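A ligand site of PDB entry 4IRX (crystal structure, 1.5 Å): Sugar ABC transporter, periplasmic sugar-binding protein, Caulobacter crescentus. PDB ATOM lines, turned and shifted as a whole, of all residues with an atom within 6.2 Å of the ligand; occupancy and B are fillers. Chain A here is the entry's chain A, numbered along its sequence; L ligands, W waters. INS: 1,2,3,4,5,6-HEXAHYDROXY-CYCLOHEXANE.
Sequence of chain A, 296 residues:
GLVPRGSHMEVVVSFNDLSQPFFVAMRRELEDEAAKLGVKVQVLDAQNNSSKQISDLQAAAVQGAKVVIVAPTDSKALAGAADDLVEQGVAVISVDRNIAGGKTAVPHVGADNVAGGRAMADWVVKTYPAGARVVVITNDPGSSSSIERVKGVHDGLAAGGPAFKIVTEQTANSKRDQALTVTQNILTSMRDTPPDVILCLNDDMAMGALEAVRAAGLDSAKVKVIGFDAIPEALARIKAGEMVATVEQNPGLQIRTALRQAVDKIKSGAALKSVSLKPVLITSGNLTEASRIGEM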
ATOM      1  N   ASN A  16      10.442   8.349 -20.477  1.00  0.00           N
ATOM      2  CA  ASN A  16      10.164   6.948 -20.189  1.00  0.00           C
ATOM      3  C   ASN A  16       9.532   6.165 -21.339  1.00  0.00           C
ATOM      4  O   ASN A  16       9.910   5.011 -21.560  1.00  0.00           O
ATOM      5  CB  ASN A  16       9.305   6.812 -18.922  1.00  0.00           C
ATOM      6  CG  ASN A  16       8.035   7.627 -18.989  1.00  0.00           C
ATOM      7  OD1 ASN A  16       8.092   8.847 -19.049  1.00  0.00           O
ATOM      8  ND2 ASN A  16       6.887   6.954 -18.946  1.00  0.00           N
ATOM      9  N   GLN A  20       3.248   7.304 -25.156  1.00  0.00           N
ATOM     10  CA  GLN A  20       2.151   7.833 -24.336  1.00  0.00           C
ATOM     11  C   GLN A  20       1.759   9.209 -24.822  1.00  0.00           C
ATOM     12  O   GLN A  20       2.608  10.093 -24.947  1.00  0.00           O
ATOM     13  CB  GLN A  20       2.555   7.955 -22.864  1.00  0.00           C
ATOM     14  CG  GLN A  20       2.840   6.640 -22.174  1.00  0.00           C
ATOM     15  CD  GLN A  20       2.953   6.777 -20.683  1.00  0.00           C
ATOM     16  OE1 GLN A  20       2.490   7.754 -20.115  1.00  0.00           O
ATOM     17  NE2 GLN A  20       3.589   5.813 -20.045  1.00  0.00           N
ATOM     18  N   PHE A  22       0.321  11.713 -23.393  1.00  0.00           N
ATOM     19  CA  PHE A  22       0.686  12.790 -22.479  1.00  0.00           C
ATOM     20  C   PHE A  22       2.089  13.257 -22.774  1.00  0.00           C
ATOM     21  O   PHE A  22       2.355  14.453 -22.788  1.00  0.00           O
ATOM     22  CB  PHE A  22       0.607  12.257 -21.058  1.00  0.00           C
ATOM     23  CG  PHE A  22       1.075  13.216 -20.005  1.00  0.00           C
ATOM     24  CD1 PHE A  22       0.226  14.193 -19.528  1.00  0.00           C
ATOM     25  CD2 PHE A  22       2.338  13.076 -19.447  1.00  0.00           C
ATOM     26  CE1 PHE A  22       0.643  15.069 -18.517  1.00  0.00           C
ATOM     27  CE2 PHE A  22       2.761  13.944 -18.413  1.00  0.00           C
ATOM     28  CZ  PHE A  22       1.894  14.929 -17.948  1.00  0.00           C
ATOM     29  N   PHE A  23       2.992  12.316 -23.025  1.00  0.00           N
ATOM     30  CA  PHE A  23       4.405  12.662 -23.221  1.00  0.00           C
ATOM     31  C   PHE A  23       4.715  13.165 -24.639  1.00  0.00           C
ATOM     32  O   PHE A  23       5.611  13.988 -24.804  1.00  0.00           O
ATOM     33  CB  PHE A  23       5.322  11.515 -22.792  1.00  0.00           C
ATOM     34  CG  PHE A  23       5.374  11.337 -21.304  1.00  0.00           C
ATOM     35  CD1 PHE A  23       5.999  12.266 -20.512  1.00  0.00           C
ATOM     36  CD2 PHE A  23       4.725  10.288 -20.690  1.00  0.00           C
ATOM     37  CE1 PHE A  23       6.023  12.105 -19.131  1.00  0.00           C
ATOM     38  CE2 PHE A  23       4.743  10.119 -19.306  1.00  0.00           C
ATOM     39  CZ  PHE A  23       5.388  11.039 -18.535  1.00  0.00           C
ATOM     40  N   ASP A  96       8.074  15.114 -14.173  1.00  0.00           N
ATOM     41  CA  ASP A  96       6.824  14.341 -14.109  1.00  0.00           C
ATOM     42  C   ASP A  96       6.757  13.330 -12.986  1.00  0.00           C
ATOM     43  O   ASP A  96       5.790  13.281 -12.217  1.00  0.00           O
ATOM     44  CB  ASP A  96       6.456  13.668 -15.429  1.00  0.00           C
ATOM     45  CG  ASP A  96       5.154  12.913 -15.311  1.00  0.00           C
ATOM     46  OD1 ASP A  96       4.092  13.587 -15.244  1.00  0.00           O
ATOM     47  OD2 ASP A  96       5.195  11.682 -15.238  1.00  0.00           O
ATOM     48  N   ARG A  97       7.779  12.484 -12.912  1.00  0.00           N
ATOM     49  CA  ARG A  97       7.946  11.558 -11.779  1.00  0.00           C
ATOM     50  C   ARG A  97       9.385  11.644 -11.279  1.00  0.00           C
ATOM     51  O   ARG A  97      10.301  12.039 -12.031  1.00  0.00           O
ATOM     52  CB  ARG A  97       7.543  10.107 -12.113  1.00  0.00           C
ATOM     53  CG  ARG A  97       8.494   9.340 -13.054  1.00  0.00           C
ATOM     54  CD  ARG A  97       8.374   9.787 -14.489  1.00  0.00           C
ATOM     55  NE  ARG A  97       7.050   9.469 -15.027  1.00  0.00           N
ATOM     56  CZ  ARG A  97       6.646   8.265 -15.446  1.00  0.00           C
ATOM     57  NH1 ARG A  97       7.463   7.222 -15.457  1.00  0.00           N
ATOM     58  NH2 ARG A  97       5.397   8.096 -15.859  1.00  0.00           N
ATOM     59  N   ASN A 113       1.318  15.022  -6.902  1.00  0.00           N
ATOM     60  CA  ASN A 113       0.442  13.923  -7.288  1.00  0.00           C
ATOM     61  C   ASN A 113      -0.394  13.367  -6.150  1.00  0.00           C
ATOM     62  O   ASN A 113      -1.500  12.853  -6.380  1.00  0.00           O
ATOM     63  CB  ASN A 113       1.256  12.845  -7.993  1.00  0.00           C
ATOM     64  CG  ASN A 113       1.515  13.191  -9.452  1.00  0.00           C
ATOM     65  OD1 ASN A 113       0.574  13.472 -10.195  1.00  0.00           O
ATOM     66  ND2 ASN A 113       2.787  13.220  -9.861  1.00  0.00           N
ATOM     67  N   ASN A 139      -1.909   4.105 -13.232  1.00  0.00           N
ATOM     68  CA  ASN A 139      -0.906   4.306 -14.272  1.00  0.00           C
ATOM     69  C   ASN A 139       0.436   3.635 -13.931  1.00  0.00           C
ATOM     70  O   ASN A 139       0.603   3.148 -12.815  1.00  0.00           O
ATOM     71  CB  ASN A 139      -0.696   5.817 -14.459  1.00  0.00           C
ATOM     72  CG  ASN A 139      -0.144   6.488 -13.213  1.00  0.00           C
ATOM     73  OD1 ASN A 139      -0.734   6.377 -12.132  1.00  0.00           O
ATOM     74  ND2 ASN A 139       0.974   7.232 -13.358  1.00  0.00           N
ATOM     75  N   ASP A 140       1.361   3.651 -14.895  1.00  0.00           N
ATOM     76  CA  ASP A 140       2.789   3.275 -14.727  1.00  0.00           C
ATOM     77  C   ASP A 140       3.227   2.874 -13.301  1.00  0.00           C
ATOM     78  O   ASP A 140       3.638   3.731 -12.515  1.00  0.00           O
ATOM     79  CB  ASP A 140       3.708   4.448 -15.168  1.00  0.00           C
ATOM     80  CG  ASP A 140       3.748   4.675 -16.661  1.00  0.00           C
ATOM     81  OD1 ASP A 140       3.736   3.710 -17.482  1.00  0.00           O
ATOM     82  OD2 ASP A 140       3.851   5.849 -17.059  1.00  0.00           O
ATOM     83  N   SER A 143       6.310   4.252 -11.334  1.00  0.00           N
ATOM     84  CA  SER A 143       6.495   5.696 -11.309  1.00  0.00           C
ATOM     85  C   SER A 143       6.046   6.311  -9.970  1.00  0.00           C
ATOM     86  O   SER A 143       5.005   5.952  -9.446  1.00  0.00           O
ATOM     87  CB  SER A 143       5.677   6.301 -12.447  1.00  0.00           C
ATOM     88  OG  SER A 143       5.662   7.717 -12.390  1.00  0.00           O
ATOM     89  N   SER A 145       4.645   8.966  -9.706  1.00  0.00           N
ATOM     90  CA  SER A 145       3.360   9.606  -9.960  1.00  0.00           C
ATOM     91  C   SER A 145       2.210   8.647  -9.672  1.00  0.00           C
ATOM     92  O   SER A 145       1.165   9.056  -9.138  1.00  0.00           O
ATOM     93  CB  SER A 145       3.282  10.158 -11.379  1.00  0.00           C
ATOM     94  OG  SER A 145       3.441   9.110 -12.311  1.00  0.00           O
ATOM     95  N   SER A 146       2.376   7.372 -10.021  1.00  0.00           N
ATOM     96  CA  SER A 146       1.370   6.361  -9.713  1.00  0.00           C
ATOM     97  C   SER A 146       1.286   6.143  -8.208  1.00  0.00           C
ATOM     98  O   SER A 146       0.209   6.179  -7.610  1.00  0.00           O
ATOM     99  CB  SER A 146       1.715   5.060 -10.411  1.00  0.00           C
ATOM    100  OG  SER A 146       0.702   4.103 -10.172  1.00  0.00           O
ATOM    101  N   ARG A 149      -0.272   9.329  -6.604  1.00  0.00           N
ATOM    102  CA  ARG A 149      -1.682   9.471  -6.955  1.00  0.00           C
ATOM    103  C   ARG A 149      -2.531   8.481  -6.210  1.00  0.00           C
ATOM    104  O   ARG A 149      -3.601   8.846  -5.701  1.00  0.00           O
ATOM    105  CB  ARG A 149      -1.931   9.271  -8.453  1.00  0.00           C
ATOM    106  CG  ARG A 149      -2.016  10.555  -9.199  1.00  0.00           C
ATOM    107  CD  ARG A 149      -2.005  10.349 -10.715  1.00  0.00           C
ATOM    108  NE  ARG A 149      -1.040  11.285 -11.258  1.00  0.00           N
ATOM    109  CZ  ARG A 149      -0.598  11.296 -12.501  1.00  0.00           C
ATOM    110  NH1 ARG A 149      -1.067  10.395 -13.372  1.00  0.00           N
ATOM    111  NH2 ARG A 149       0.329  12.160 -12.870  1.00  0.00           N
ATOM    112  N   SER A 174      -0.728   2.429 -18.003  1.00  0.00           N
ATOM    113  CA  SER A 174      -0.816   3.622 -18.859  1.00  0.00           C
ATOM    114  C   SER A 174      -1.047   3.268 -20.333  1.00  0.00           C
ATOM    115  O   SER A 174      -0.464   3.867 -21.244  1.00  0.00           O
ATOM    116  CB  SER A 174       0.455   4.491 -18.702  1.00  0.00           C
ATOM    117  OG  SER A 174       0.530   5.044 -17.385  1.00  0.00           O
ATOM    118  N   LEU A 201      -6.119   6.796 -13.471  1.00  0.00           N
ATOM    119  CA  LEU A 201      -5.013   7.689 -13.145  1.00  0.00           C
ATOM    120  C   LEU A 201      -4.288   8.266 -14.360  1.00  0.00           C
ATOM    121  O   LEU A 201      -3.241   8.915 -14.248  1.00  0.00           O
ATOM    122  CB  LEU A 201      -4.068   7.023 -12.139  1.00  0.00           C
ATOM    123  CG  LEU A 201      -4.507   7.138 -10.661  1.00  0.00           C
ATOM    124  CD1 LEU A 201      -5.941   6.752 -10.377  1.00  0.00           C
ATOM    125  CD2 LEU A 201      -3.569   6.313  -9.817  1.00  0.00           C
ATOM    126  N   ASN A 202      -4.849   8.065 -15.558  1.00  0.00           N
ATOM    127  CA  ASN A 202      -4.581   8.963 -16.681  1.00  0.00           C
ATOM    128  C   ASN A 202      -5.753   8.973 -17.651  1.00  0.00           C
ATOM    129  O   ASN A 202      -6.627   8.098 -17.579  1.00  0.00           O
ATOM    130  CB  ASN A 202      -3.196   8.747 -17.366  1.00  0.00           C
ATOM    131  CG  ASN A 202      -3.177   7.606 -18.358  1.00  0.00           C
ATOM    132  OD1 ASN A 202      -4.165   6.925 -18.584  1.00  0.00           O
ATOM    133  ND2 ASN A 202      -2.030   7.400 -18.977  1.00  0.00           N
ATOM    134  N   ASP A 203      -5.770   9.958 -18.525  1.00  0.00           N
ATOM    135  CA  ASP A 203      -6.913  10.148 -19.438  1.00  0.00           C
ATOM    136  C   ASP A 203      -6.926   9.109 -20.552  1.00  0.00           C
ATOM    137  O   ASP A 203      -7.986   8.712 -20.991  1.00  0.00           O
ATOM    138  CB  ASP A 203      -6.890  11.536 -20.081  1.00  0.00           C
ATOM    139  CG  ASP A 203      -7.376  12.631 -19.147  1.00  0.00           C
ATOM    140  OD1 ASP A 203      -8.103  12.335 -18.163  1.00  0.00           O
ATOM    141  OD2 ASP A 203      -7.014  13.793 -19.446  1.00  0.00           O
ATOM    142  N   ASP A 204      -5.751   8.674 -20.988  1.00  0.00           N
ATOM    143  CA  ASP A 204      -5.641   7.630 -22.031  1.00  0.00           C
ATOM    144  C   ASP A 204      -6.363   6.359 -21.562  1.00  0.00           C
ATOM    145  O   ASP A 204      -7.164   5.773 -22.301  1.00  0.00           O
ATOM    146  CB  ASP A 204      -4.145   7.376 -22.318  1.00  0.00           C
ATOM    147  CG  ASP A 204      -3.881   6.713 -23.683  1.00  0.00           C
ATOM    148  OD1 ASP A 204      -4.710   6.831 -24.620  1.00  0.00           O
ATOM    149  OD2 ASP A 204      -2.815   6.075 -23.814  1.00  0.00           O
ATOM    150  N   MET A 205      -6.103   5.956 -20.325  1.00  0.00           N
ATOM    151  CA  MET A 205      -6.790   4.808 -19.740  1.00  0.00           C
ATOM    152  C   MET A 205      -8.252   5.109 -19.503  1.00  0.00           C
ATOM    153  O   MET A 205      -9.092   4.220 -19.672  1.00  0.00           O
ATOM    154  CB  MET A 205      -6.132   4.383 -18.416  1.00  0.00           C
ATOM    155  CG  MET A 205      -4.706   3.817 -18.580  1.00  0.00           C
ATOM    156  SD  MET A 205      -3.980   3.172 -16.913  1.00  0.00           S
ATOM    157  CE  MET A 205      -4.083   4.831 -15.879  1.00  0.00           C
ATOM    158  N   PHE A 228      -7.184  11.808 -15.409  1.00  0.00           N
ATOM    159  CA  PHE A 228      -6.074  12.632 -14.957  1.00  0.00           C
ATOM    160  C   PHE A 228      -5.284  12.975 -16.204  1.00  0.00           C
ATOM    161  O   PHE A 228      -4.952  12.084 -16.983  1.00  0.00           O
ATOM    162  CB  PHE A 228      -5.202  11.833 -13.966  1.00  0.00           C
ATOM    163  CG  PHE A 228      -4.376  12.686 -13.016  1.00  0.00           C
ATOM    164  CD1 PHE A 228      -3.262  13.385 -13.484  1.00  0.00           C
ATOM    165  CD2 PHE A 228      -4.710  12.780 -11.671  1.00  0.00           C
ATOM    166  CE1 PHE A 228      -2.480  14.180 -12.596  1.00  0.00           C
ATOM    167  CE2 PHE A 228      -3.950  13.544 -10.771  1.00  0.00           C
ATOM    168  CZ  PHE A 228      -2.823  14.262 -11.235  1.00  0.00           C
ATOM    169  N   ASP A 229      -4.992  14.260 -16.406  1.00  0.00           N
ATOM    170  CA  ASP A 229      -4.085  14.826 -17.461  1.00  0.00           C
ATOM    171  C   ASP A 229      -4.718  15.982 -18.221  1.00  0.00           C
ATOM    172  O   ASP A 229      -4.003  16.813 -18.755  1.00  0.00           O
ATOM    173  CB  ASP A 229      -3.540  13.842 -18.531  1.00  0.00           C
ATOM    174  CG  ASP A 229      -2.557  12.846 -17.987  1.00  0.00           C
ATOM    175  OD1 ASP A 229      -2.041  13.060 -16.871  1.00  0.00           O
ATOM    176  OD2 ASP A 229      -2.303  11.830 -18.666  1.00  0.00           O
ATOM    177  N   GLN A 249      -2.573  19.128 -14.660  1.00  0.00           N
ATOM    178  CA  GLN A 249      -1.275  19.110 -13.986  1.00  0.00           C
ATOM    179  C   GLN A 249      -0.186  19.924 -14.696  1.00  0.00           C
ATOM    180  O   GLN A 249       1.002  19.866 -14.323  1.00  0.00           O
ATOM    181  CB  GLN A 249      -0.783  17.689 -13.771  1.00  0.00           C
ATOM    182  CG  GLN A 249      -0.589  16.842 -15.010  1.00  0.00           C
ATOM    183  CD  GLN A 249       0.320  15.662 -14.748  1.00  0.00           C
ATOM    184  OE1 GLN A 249       1.331  15.777 -14.039  1.00  0.00           O
ATOM    185  NE2 GLN A 249      -0.071  14.482 -15.281  1.00  0.00           N
ATOM    186  N   GLN A 254       5.701  22.117 -16.456  1.00  0.00           N
ATOM    187  CA  GLN A 254       6.708  21.218 -15.881  1.00  0.00           C
ATOM    188  C   GLN A 254       7.957  21.158 -16.733  1.00  0.00           C
ATOM    189  O   GLN A 254       9.068  21.362 -16.242  1.00  0.00           O
ATOM    190  CB  GLN A 254       6.164  19.796 -15.724  1.00  0.00           C
ATOM    191  CG  GLN A 254       5.033  19.656 -14.687  1.00  0.00           C
ATOM    192  CD  GLN A 254       4.568  18.224 -14.547  1.00  0.00           C
ATOM    193  OE1 GLN A 254       5.373  17.285 -14.472  1.00  0.00           O
ATOM    194  NE2 GLN A 254       3.237  18.033 -14.565  1.00  0.00           N
HETATM  195  C1  INS L   1       1.912  11.264 -16.179  1.00  0.00           C
HETATM  196  C2  INS L   1       0.651  11.212 -16.973  1.00  0.00           C
HETATM  197  C3  INS L   1       0.738  10.068 -17.951  1.00  0.00           C
HETATM  198  C4  INS L   1       0.902   8.775 -17.222  1.00  0.00           C
HETATM  199  C5  INS L   1       2.173   8.783 -16.458  1.00  0.00           C
HETATM  200  C6  INS L   1       2.227   9.938 -15.500  1.00  0.00           C
HETATM  201  O1  INS L   1       1.853  12.299 -15.235  1.00  0.00           O
HETATM  202  O2  INS L   1      -0.436  11.064 -16.108  1.00  0.00           O
HETATM  203  O3  INS L   1      -0.396  10.043 -18.778  1.00  0.00           O
HETATM  204  O4  INS L   1       0.848   7.702 -18.100  1.00  0.00           O
HETATM  205  O5  INS L   1       2.307   7.564 -15.790  1.00  0.00           O
HETATM  206  O6  INS L   1       3.416   9.947 -14.748  1.00  0.00           O
HETATM  207  O   HOH W   1      -0.665   9.353 -21.629  1.00  0.00           O
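An oxygen (O6) of the ligand lies within hydrogen-bond range of the side-chain carboxylate (OD2) of Asp 96 (2.5 Å).
An oxygen (O6) of the ligand lies within hydrogen-bond range of the side-chain hydroxyl (OG) of Ser 145 (2.6 Å).
OE1 of Gln 20 sits at hydrogen-bond distance from O4 of the ligand (2.6 Å).
O3 of the ligand lies within hydrogen-bond range of OD2 of Asp 229 (2.6 Å).
OD2 of Asp 140 lies within hydrogen-bond range of O5 of the ligand (2.6 Å).
OG of Ser 174 is in hydrogen-bond range of O4 of the ligand (2.8 Å).
O5 of the ligand lies within hydrogen-bond range of ND2 of Asn 139 (2.8 Å).
O1 of the ligand sits at hydrogen-bond distance from NH2 of Arg 149 (2.8 Å).
An oxygen (O1) of the ligand sits at hydrogen-bond distance from the side-chain amide nitrogen (NE2) of Gln 249 (2.9 Å).
The guanidinium group of Arg 97 lies within hydrogen-bond range of an oxygen (O6) of the ligand.
The side-chain amide nitrogen of Asn 202 lies within hydrogen-bond range of an oxygen (O4) of the ligand, 3.0 Å away.
OD2 of Asp 96 is in salt-bridge range of NE of Arg 97 (2.9 Å).
The backbone NH of Asp 96 lies close to the side-chain amide oxygen of Gln 254, at 3.5 Å.
The side-chain hydroxyl (OG) of Ser 145 sits at hydrogen-bond distance from the side-chain hydroxyl (OG) of Ser 143.
NE2 of Gln 20 sits at hydrogen-bond distance from OD2 of Asp 140, at 3.0 Å.
The backbone NH (N) of Ser 174 lies within hydrogen-bond range of the side-chain sulfur (SD) of Met 205 (3.5 Å).
The side-chain amide oxygen (OD1) of Asn 113 sits at hydrogen-bond distance from the guanidinium group (NE) of Arg 149, 2.9 Å away.
The backbone carbonyl oxygen of Gln 249 sits at hydrogen-bond distance from the side-chain amide nitrogen of Gln 254 (2.9 Å).
The guanidinium group of Arg 97 lies close to the side-chain hydroxyl of Ser 143 (3.5 Å).
CB of Phe 22 touches O3 of the ligand, 3.3 Å away.
OG of Ser 143 touches O6 of the ligand, at 3.9 Å.
Leu 201 touches the ligand (O to O2, 3.99 Å).
Hydrophobic or aromatic side chains within 4 Å of the ligand: Phe 22.
Within 4 Å of the ligand: Gln 20, Phe 22, Asp 96, Arg 97, Asn 139, Asp 140, Ser 143, Ser 145, Arg 149, Ser 174, Leu 201, Asn 202, Asp 229 and Gln 249.
Along chain A the residues within 4 Å of the ligand span positions 20 to 249.
The nearest printed residue that does not touch the ligand is Phe 23 (4.1 Å).
Water W1 lies within hydrogen-bond range of O3 of the ligand (2.9 Å) and N of Phe 22 (3.1 Å).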
